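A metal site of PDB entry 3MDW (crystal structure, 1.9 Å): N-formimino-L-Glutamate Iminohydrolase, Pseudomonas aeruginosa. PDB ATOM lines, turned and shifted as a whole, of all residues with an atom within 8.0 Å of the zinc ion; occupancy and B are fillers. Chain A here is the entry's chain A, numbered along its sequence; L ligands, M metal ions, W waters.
A nitrogen (N2) of the ligand lies within salt-bridge range of the side-chain carboxylate (OD2) of Asp 320 (3.6 Å). N2 of the ligand lies within salt-bridge range of OE2 of Glu 235. An oxygen (O1) of the ligand sits at hydrogen-bond distance from the side-chain hydroxyl of Tyr 121, at 2.7 Å. NE2 of Gln 61 is in hydrogen-bond range of O1 of the ligand (3.1 Å). NE2 of His 206 sits at hydrogen-bond distance from O2 of the ligand, 2.7 Å away.
Water W1 lies within hydrogen-bond range of the side-chain carboxylate of Asp 320 (2.5 Å), a ring nitrogen (NE2) of His 269 (2.6 Å) and a nitrogen (N2) of the ligand (2.8 Å).
The zinc ion is bound by water W1. The zinc ion is bound by NE2 of His 58 (2.1 Å). NE2 of His 56 is bound to the zinc ion, 2.1 Å away. A ring nitrogen (NE2) of His 232 is bound to the zinc ion. Slightly farther from the zinc ion lies OD1 of Asp 320 (2.8 Å).
O of Asp 320 is in hydrogen-bond range of N of His 58 (3.1 Å). A ring nitrogen (ND1) of His 58 sits at hydrogen-bond distance from the backbone carbonyl oxygen (O) of Phe 119 (2.9 Å). The backbone NH (N) of Asp 320 is in hydrogen-bond range of the backbone carbonyl oxygen (O) of His 56 (2.8 Å). The backbone carbonyl oxygen (O) of His 56 is in hydrogen-bond range of the backbone NH (N) of Ser 319 (3.3 Å). ND1 of His 232 is in hydrogen-bond range of O of His 206 (2.9 Å). A ring nitrogen (NE2) of His 269 lies close to the side-chain carboxylate of Asp 320. The side-chain carboxylate (OE1) of Glu 235 lies close to a ring nitrogen (NE2) of His 269, at 3.4 Å. O of Gly 289 is in hydrogen-bond range of N of His 269, at 2.7 Å.
His 269 touches the zinc ion. The nearest printed residue that does not touch the zinc ion is Val 268 (4.7 Å).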
ATOM      1  N   HIS A  56       1.938   2.990  -0.318  1.00  0.00           N
ATOM      2  CA  HIS A  56       2.432   4.300  -0.724  1.00  0.00           C
ATOM      3  C   HIS A  56       2.240   5.399   0.340  1.00  0.00           C
ATOM      4  O   HIS A  56       1.098   5.714   0.708  1.00  0.00           O
ATOM      5  CB  HIS A  56       1.787   4.726  -2.047  1.00  0.00           C
ATOM      6  CG  HIS A  56       2.395   5.949  -2.644  1.00  0.00           C
ATOM      7  ND1 HIS A  56       3.651   5.960  -3.210  1.00  0.00           N
ATOM      8  CD2 HIS A  56       1.914   7.214  -2.787  1.00  0.00           C
ATOM      9  CE1 HIS A  56       3.928   7.167  -3.662  1.00  0.00           C
ATOM     10  NE2 HIS A  56       2.898   7.953  -3.419  1.00  0.00           N
ATOM     11  N   SER A  57       3.345   5.988   0.793  1.00  0.00           N
ATOM     12  CA  SER A  57       3.281   7.002   1.855  1.00  0.00           C
ATOM     13  C   SER A  57       4.363   8.085   1.746  1.00  0.00           C
ATOM     14  O   SER A  57       5.510   7.789   1.424  1.00  0.00           O
ATOM     15  CB  SER A  57       3.423   6.307   3.221  1.00  0.00           C
ATOM     16  OG  SER A  57       3.873   7.203   4.222  1.00  0.00           O
ATOM     17  N   HIS A  58       3.998   9.344   2.009  1.00  0.00           N
ATOM     18  CA  HIS A  58       5.007  10.392   2.258  1.00  0.00           C
ATOM     19  C   HIS A  58       4.789  10.936   3.671  1.00  0.00           C
ATOM     20  O   HIS A  58       3.951  11.828   3.875  1.00  0.00           O
ATOM     21  CB  HIS A  58       4.882  11.556   1.260  1.00  0.00           C
ATOM     22  CG  HIS A  58       4.790  11.119  -0.169  1.00  0.00           C
ATOM     23  ND1 HIS A  58       5.794  10.421  -0.808  1.00  0.00           N
ATOM     24  CD2 HIS A  58       3.808  11.301  -1.086  1.00  0.00           C
ATOM     25  CE1 HIS A  58       5.433  10.176  -2.058  1.00  0.00           C
ATOM     26  NE2 HIS A  58       4.241  10.718  -2.260  1.00  0.00           N
ATOM     27  N   GLN A  61       3.834  14.564   5.145  1.00  0.00           N
ATOM     28  CA  GLN A  61       2.608  15.220   4.697  1.00  0.00           C
ATOM     29  C   GLN A  61       1.447  15.106   5.690  1.00  0.00           C
ATOM     30  O   GLN A  61       0.538  15.939   5.675  1.00  0.00           O
ATOM     31  CB  GLN A  61       2.199  14.736   3.295  1.00  0.00           C
ATOM     32  CG  GLN A  61       3.272  15.063   2.250  1.00  0.00           C
ATOM     33  CD  GLN A  61       2.855  14.721   0.826  1.00  0.00           C
ATOM     34  OE1 GLN A  61       1.713  14.368   0.559  1.00  0.00           O
ATOM     35  NE2 GLN A  61       3.811  14.845  -0.089  1.00  0.00           N
ATOM     36  N   PHE A  78      -3.991  20.414  -7.878  1.00  0.00           N
ATOM     37  CA  PHE A  78      -2.812  19.649  -7.506  1.00  0.00           C
ATOM     38  C   PHE A  78      -1.573  20.550  -7.492  1.00  0.00           C
ATOM     39  O   PHE A  78      -0.744  20.456  -6.599  1.00  0.00           O
ATOM     40  CB  PHE A  78      -2.646  18.511  -8.526  1.00  0.00           C
ATOM     41  CG  PHE A  78      -1.347  17.764  -8.440  1.00  0.00           C
ATOM     42  CD1 PHE A  78      -1.300  16.503  -7.848  1.00  0.00           C
ATOM     43  CD2 PHE A  78      -0.187  18.286  -8.987  1.00  0.00           C
ATOM     44  CE1 PHE A  78      -0.095  15.798  -7.782  1.00  0.00           C
ATOM     45  CE2 PHE A  78       1.016  17.595  -8.925  1.00  0.00           C
ATOM     46  CZ  PHE A  78       1.065  16.338  -8.319  1.00  0.00           C
ATOM     47  N   TRP A  81      -1.554  23.094  -4.699  1.00  0.00           N
ATOM     48  CA  TRP A  81      -1.341  22.314  -3.475  1.00  0.00           C
ATOM     49  C   TRP A  81       0.143  22.012  -3.310  1.00  0.00           C
ATOM     50  O   TRP A  81       0.687  22.121  -2.204  1.00  0.00           O
ATOM     51  CB  TRP A  81      -2.132  21.008  -3.509  1.00  0.00           C
ATOM     52  CG  TRP A  81      -1.716  20.020  -2.442  1.00  0.00           C
ATOM     53  CD1 TRP A  81      -2.218  19.915  -1.165  1.00  0.00           C
ATOM     54  CD2 TRP A  81      -0.714  18.991  -2.558  1.00  0.00           C
ATOM     55  NE1 TRP A  81      -1.589  18.895  -0.488  1.00  0.00           N
ATOM     56  CE2 TRP A  81      -0.659  18.316  -1.310  1.00  0.00           C
ATOM     57  CE3 TRP A  81       0.127  18.581  -3.590  1.00  0.00           C
ATOM     58  CZ2 TRP A  81       0.207  17.243  -1.079  1.00  0.00           C
ATOM     59  CZ3 TRP A  81       1.005  17.514  -3.347  1.00  0.00           C
ATOM     60  CH2 TRP A  81       1.035  16.854  -2.107  1.00  0.00           C
ATOM     61  N   PHE A 119       7.718   6.187   0.542  1.00  0.00           N
ATOM     62  CA  PHE A 119       8.215   6.695  -0.722  1.00  0.00           C
ATOM     63  C   PHE A 119       8.931   7.979  -0.333  1.00  0.00           C
ATOM     64  O   PHE A 119       8.324   9.038  -0.227  1.00  0.00           O
ATOM     65  CB  PHE A 119       6.987   6.946  -1.624  1.00  0.00           C
ATOM     66  CG  PHE A 119       7.290   7.182  -3.078  1.00  0.00           C
ATOM     67  CD1 PHE A 119       7.840   8.388  -3.501  1.00  0.00           C
ATOM     68  CD2 PHE A 119       6.927   6.242  -4.034  1.00  0.00           C
ATOM     69  CE1 PHE A 119       8.066   8.631  -4.858  1.00  0.00           C
ATOM     70  CE2 PHE A 119       7.144   6.482  -5.389  1.00  0.00           C
ATOM     71  CZ  PHE A 119       7.708   7.681  -5.797  1.00  0.00           C
ATOM     72  N   TYR A 121      11.529  10.935  -0.303  1.00  0.00           N
ATOM     73  CA  TYR A 121      12.349  11.813  -1.141  1.00  0.00           C
ATOM     74  C   TYR A 121      12.926  13.037  -0.437  1.00  0.00           C
ATOM     75  O   TYR A 121      13.577  13.860  -1.067  1.00  0.00           O
ATOM     76  CB  TYR A 121      11.580  12.267  -2.388  1.00  0.00           C
ATOM     77  CG  TYR A 121      10.230  12.888  -2.080  1.00  0.00           C
ATOM     78  CD1 TYR A 121      10.150  14.131  -1.453  1.00  0.00           C
ATOM     79  CD2 TYR A 121       9.051  12.249  -2.421  1.00  0.00           C
ATOM     80  CE1 TYR A 121       8.936  14.715  -1.168  1.00  0.00           C
ATOM     81  CE2 TYR A 121       7.813  12.832  -2.155  1.00  0.00           C
ATOM     82  CZ  TYR A 121       7.768  14.062  -1.522  1.00  0.00           C
ATOM     83  OH  TYR A 121       6.561  14.662  -1.243  1.00  0.00           O
ATOM     84  N   HIS A 206      11.114   9.171  -8.611  1.00  0.00           N
ATOM     85  CA  HIS A 206       9.991   9.979  -8.184  1.00  0.00           C
ATOM     86  C   HIS A 206       8.882   9.976  -9.234  1.00  0.00           C
ATOM     87  O   HIS A 206       7.705   9.791  -8.914  1.00  0.00           O
ATOM     88  CB  HIS A 206      10.389  11.416  -7.865  1.00  0.00           C
ATOM     89  CG  HIS A 206       9.215  12.285  -7.543  1.00  0.00           C
ATOM     90  ND1 HIS A 206       8.491  12.957  -8.507  1.00  0.00           N
ATOM     91  CD2 HIS A 206       8.582  12.537  -6.365  1.00  0.00           C
ATOM     92  CE1 HIS A 206       7.502  13.613  -7.933  1.00  0.00           C
ATOM     93  NE2 HIS A 206       7.532  13.375  -6.635  1.00  0.00           N
ATOM     94  N   ILE A 231       7.282   4.098  -8.813  1.00  0.00           N
ATOM     95  CA  ILE A 231       7.335   5.385  -9.514  1.00  0.00           C
ATOM     96  C   ILE A 231       5.935   6.034  -9.509  1.00  0.00           C
ATOM     97  O   ILE A 231       4.944   5.340  -9.663  1.00  0.00           O
ATOM     98  CB  ILE A 231       7.811   5.195 -10.983  1.00  0.00           C
ATOM     99  CG1 ILE A 231       7.990   6.541 -11.672  1.00  0.00           C
ATOM    100  CG2 ILE A 231       6.845   4.332 -11.781  1.00  0.00           C
ATOM    101  CD1 ILE A 231       8.773   6.458 -12.997  1.00  0.00           C
ATOM    102  N   HIS A 232       5.856   7.354  -9.316  1.00  0.00           N
ATOM    103  CA  HIS A 232       4.597   8.058  -9.559  1.00  0.00           C
ATOM    104  C   HIS A 232       4.419   8.156 -11.065  1.00  0.00           C
ATOM    105  O   HIS A 232       5.354   8.520 -11.761  1.00  0.00           O
ATOM    106  CB  HIS A 232       4.630   9.505  -9.082  1.00  0.00           C
ATOM    107  CG  HIS A 232       4.629   9.696  -7.605  1.00  0.00           C
ATOM    108  ND1 HIS A 232       5.665  10.313  -6.936  1.00  0.00           N
ATOM    109  CD2 HIS A 232       3.697   9.396  -6.668  1.00  0.00           C
ATOM    110  CE1 HIS A 232       5.375  10.375  -5.644  1.00  0.00           C
ATOM    111  NE2 HIS A 232       4.195   9.824  -5.455  1.00  0.00           N
ATOM    112  N   GLU A 235      -0.524  10.643 -12.758  1.00  0.00           N
ATOM    113  CA  GLU A 235      -1.459  11.145 -11.752  1.00  0.00           C
ATOM    114  C   GLU A 235      -2.302  12.329 -12.259  1.00  0.00           C
ATOM    115  O   GLU A 235      -3.505  12.396 -12.009  1.00  0.00           O
ATOM    116  CB  GLU A 235      -0.734  11.538 -10.457  1.00  0.00           C
ATOM    117  CG  GLU A 235      -1.691  11.897  -9.315  1.00  0.00           C
ATOM    118  CD  GLU A 235      -0.997  12.332  -8.035  1.00  0.00           C
ATOM    119  OE1 GLU A 235       0.235  12.525  -8.055  1.00  0.00           O
ATOM    120  OE2 GLU A 235      -1.695  12.463  -6.993  1.00  0.00           O
ATOM    121  N   VAL A 268       2.446   4.066  -9.133  1.00  0.00           N
ATOM    122  CA  VAL A 268       1.585   4.782  -8.201  1.00  0.00           C
ATOM    123  C   VAL A 268       0.647   5.727  -8.942  1.00  0.00           C
ATOM    124  O   VAL A 268       1.060   6.452  -9.839  1.00  0.00           O
ATOM    125  CB  VAL A 268       2.420   5.537  -7.142  1.00  0.00           C
ATOM    126  CG1 VAL A 268       1.516   6.234  -6.126  1.00  0.00           C
ATOM    127  CG2 VAL A 268       3.357   4.571  -6.425  1.00  0.00           C
ATOM    128  N   HIS A 269      -0.626   5.693  -8.553  1.00  0.00           N
ATOM    129  CA  HIS A 269      -1.727   6.414  -9.212  1.00  0.00           C
ATOM    130  C   HIS A 269      -2.128   5.818 -10.564  1.00  0.00           C
ATOM    131  O   HIS A 269      -3.207   5.244 -10.693  1.00  0.00           O
ATOM    132  CB  HIS A 269      -1.420   7.914  -9.333  1.00  0.00           C
ATOM    133  CG  HIS A 269      -0.993   8.538  -8.044  1.00  0.00           C
ATOM    134  ND1 HIS A 269      -1.783   8.515  -6.912  1.00  0.00           N
ATOM    135  CD2 HIS A 269       0.146   9.178  -7.690  1.00  0.00           C
ATOM    136  CE1 HIS A 269      -1.160   9.120  -5.917  1.00  0.00           C
ATOM    137  NE2 HIS A 269       0.017   9.536  -6.365  1.00  0.00           N
ATOM    138  N   GLY A 289      -0.709   1.318  -7.829  1.00  0.00           N
ATOM    139  CA  GLY A 289      -0.797   1.825  -6.475  1.00  0.00           C
ATOM    140  C   GLY A 289      -1.843   2.903  -6.329  1.00  0.00           C
ATOM    141  O   GLY A 289      -1.563   4.081  -6.561  1.00  0.00           O
ATOM    142  N   CYS A 291      -4.367   5.435  -4.543  1.00  0.00           N
ATOM    143  CA  CYS A 291      -4.468   6.196  -3.299  1.00  0.00           C
ATOM    144  C   CYS A 291      -5.726   7.033  -3.415  1.00  0.00           C
ATOM    145  O   CYS A 291      -5.702   8.205  -3.816  1.00  0.00           O
ATOM    146  CB  CYS A 291      -3.230   7.078  -3.140  1.00  0.00           C
ATOM    147  SG  CYS A 291      -1.673   6.131  -3.354  1.00  0.00           S
ATOM    148  N   THR A 294      -6.399  10.462  -1.373  1.00  0.00           N
ATOM    149  CA  THR A 294      -5.520  11.534  -1.814  1.00  0.00           C
ATOM    150  C   THR A 294      -5.855  11.965  -3.246  1.00  0.00           C
ATOM    151  O   THR A 294      -5.898  13.154  -3.547  1.00  0.00           O
ATOM    152  CB  THR A 294      -4.026  11.145  -1.679  1.00  0.00           C
ATOM    153  OG1 THR A 294      -3.650  11.153  -0.286  1.00  0.00           O
ATOM    154  CG2 THR A 294      -3.144  12.149  -2.448  1.00  0.00           C
ATOM    155  N   LEU A 298      -6.854  15.682  -4.135  1.00  0.00           N
ATOM    156  CA  LEU A 298      -6.069  16.477  -5.072  1.00  0.00           C
ATOM    157  C   LEU A 298      -6.721  16.720  -6.442  1.00  0.00           C
ATOM    158  O   LEU A 298      -6.136  17.361  -7.318  1.00  0.00           O
ATOM    159  CB  LEU A 298      -4.678  15.845  -5.280  1.00  0.00           C
ATOM    160  CG  LEU A 298      -3.834  15.750  -4.020  1.00  0.00           C
ATOM    161  CD1 LEU A 298      -2.495  15.086  -4.315  1.00  0.00           C
ATOM    162  CD2 LEU A 298      -3.621  17.157  -3.440  1.00  0.00           C
ATOM    163  N   SER A 319      -2.095   5.420   1.465  1.00  0.00           N
ATOM    164  CA  SER A 319      -2.694   6.628   2.039  1.00  0.00           C
ATOM    165  C   SER A 319      -2.003   7.928   1.572  1.00  0.00           C
ATOM    166  O   SER A 319      -2.552   9.014   1.737  1.00  0.00           O
ATOM    167  CB  SER A 319      -2.722   6.559   3.574  1.00  0.00           C
ATOM    168  OG  SER A 319      -1.413   6.459   4.100  1.00  0.00           O
ATOM    169  N   ASP A 320      -0.783   7.810   1.024  1.00  0.00           N
ATOM    170  CA  ASP A 320      -0.117   8.879   0.259  1.00  0.00           C
ATOM    171  C   ASP A 320       0.099  10.207   1.008  1.00  0.00           C
ATOM    172  O   ASP A 320       1.068  10.339   1.755  1.00  0.00           O
ATOM    173  CB  ASP A 320      -0.853   9.106  -1.072  1.00  0.00           C
ATOM    174  CG  ASP A 320      -0.077  10.010  -2.014  1.00  0.00           C
ATOM    175  OD1 ASP A 320       1.084  10.362  -1.705  1.00  0.00           O
ATOM    176  OD2 ASP A 320      -0.622  10.369  -3.082  1.00  0.00           O
ATOM    177  N   SER A 321      -0.788  11.184   0.797  1.00  0.00           N
ATOM    178  CA  SER A 321      -0.685  12.471   1.506  1.00  0.00           C
ATOM    179  C   SER A 321      -1.232  12.359   2.923  1.00  0.00           C
ATOM    180  O   SER A 321      -1.105  13.292   3.714  1.00  0.00           O
ATOM    181  CB  SER A 321      -1.408  13.592   0.748  1.00  0.00           C
ATOM    182  OG  SER A 321      -2.817  13.457   0.865  1.00  0.00           O
HETATM  183  C1  LIG L   1       4.813  14.200  -4.202  1.00  0.00           C
HETATM  184  N1  LIG L   1       2.406  14.070  -4.635  1.00  0.00           N
HETATM  185  O1  LIG L   1       4.526  14.165  -2.980  1.00  0.00           O
HETATM  186  O2  LIG L   1       6.009  14.250  -4.548  1.00  0.00           O
HETATM  187  C2  LIG L   1       3.723  14.180  -5.279  1.00  0.00           C
HETATM  188  C3  LIG L   1       3.838  15.443  -6.167  1.00  0.00           C
HETATM  189  C4  LIG L   1       1.199  13.692  -5.389  1.00  0.00           C
HETATM  190  N2  LIG L   1       0.139  13.439  -4.771  1.00  0.00           N
HETATM  191  C5  LIG L   1       4.547  15.177  -7.507  1.00  0.00           C
HETATM  192  O3  LIG L   1       4.257  14.147  -8.154  1.00  0.00           O
HETATM  193  O4  LIG L   1       5.367  16.029  -7.918  1.00  0.00           O
HETATM  194 ZN    ZN M   1       2.947  10.004  -3.702  1.00  0.00          ZN
HETATM  195  O   HOH W   1       1.328  10.887  -4.621  1.00  0.00           O
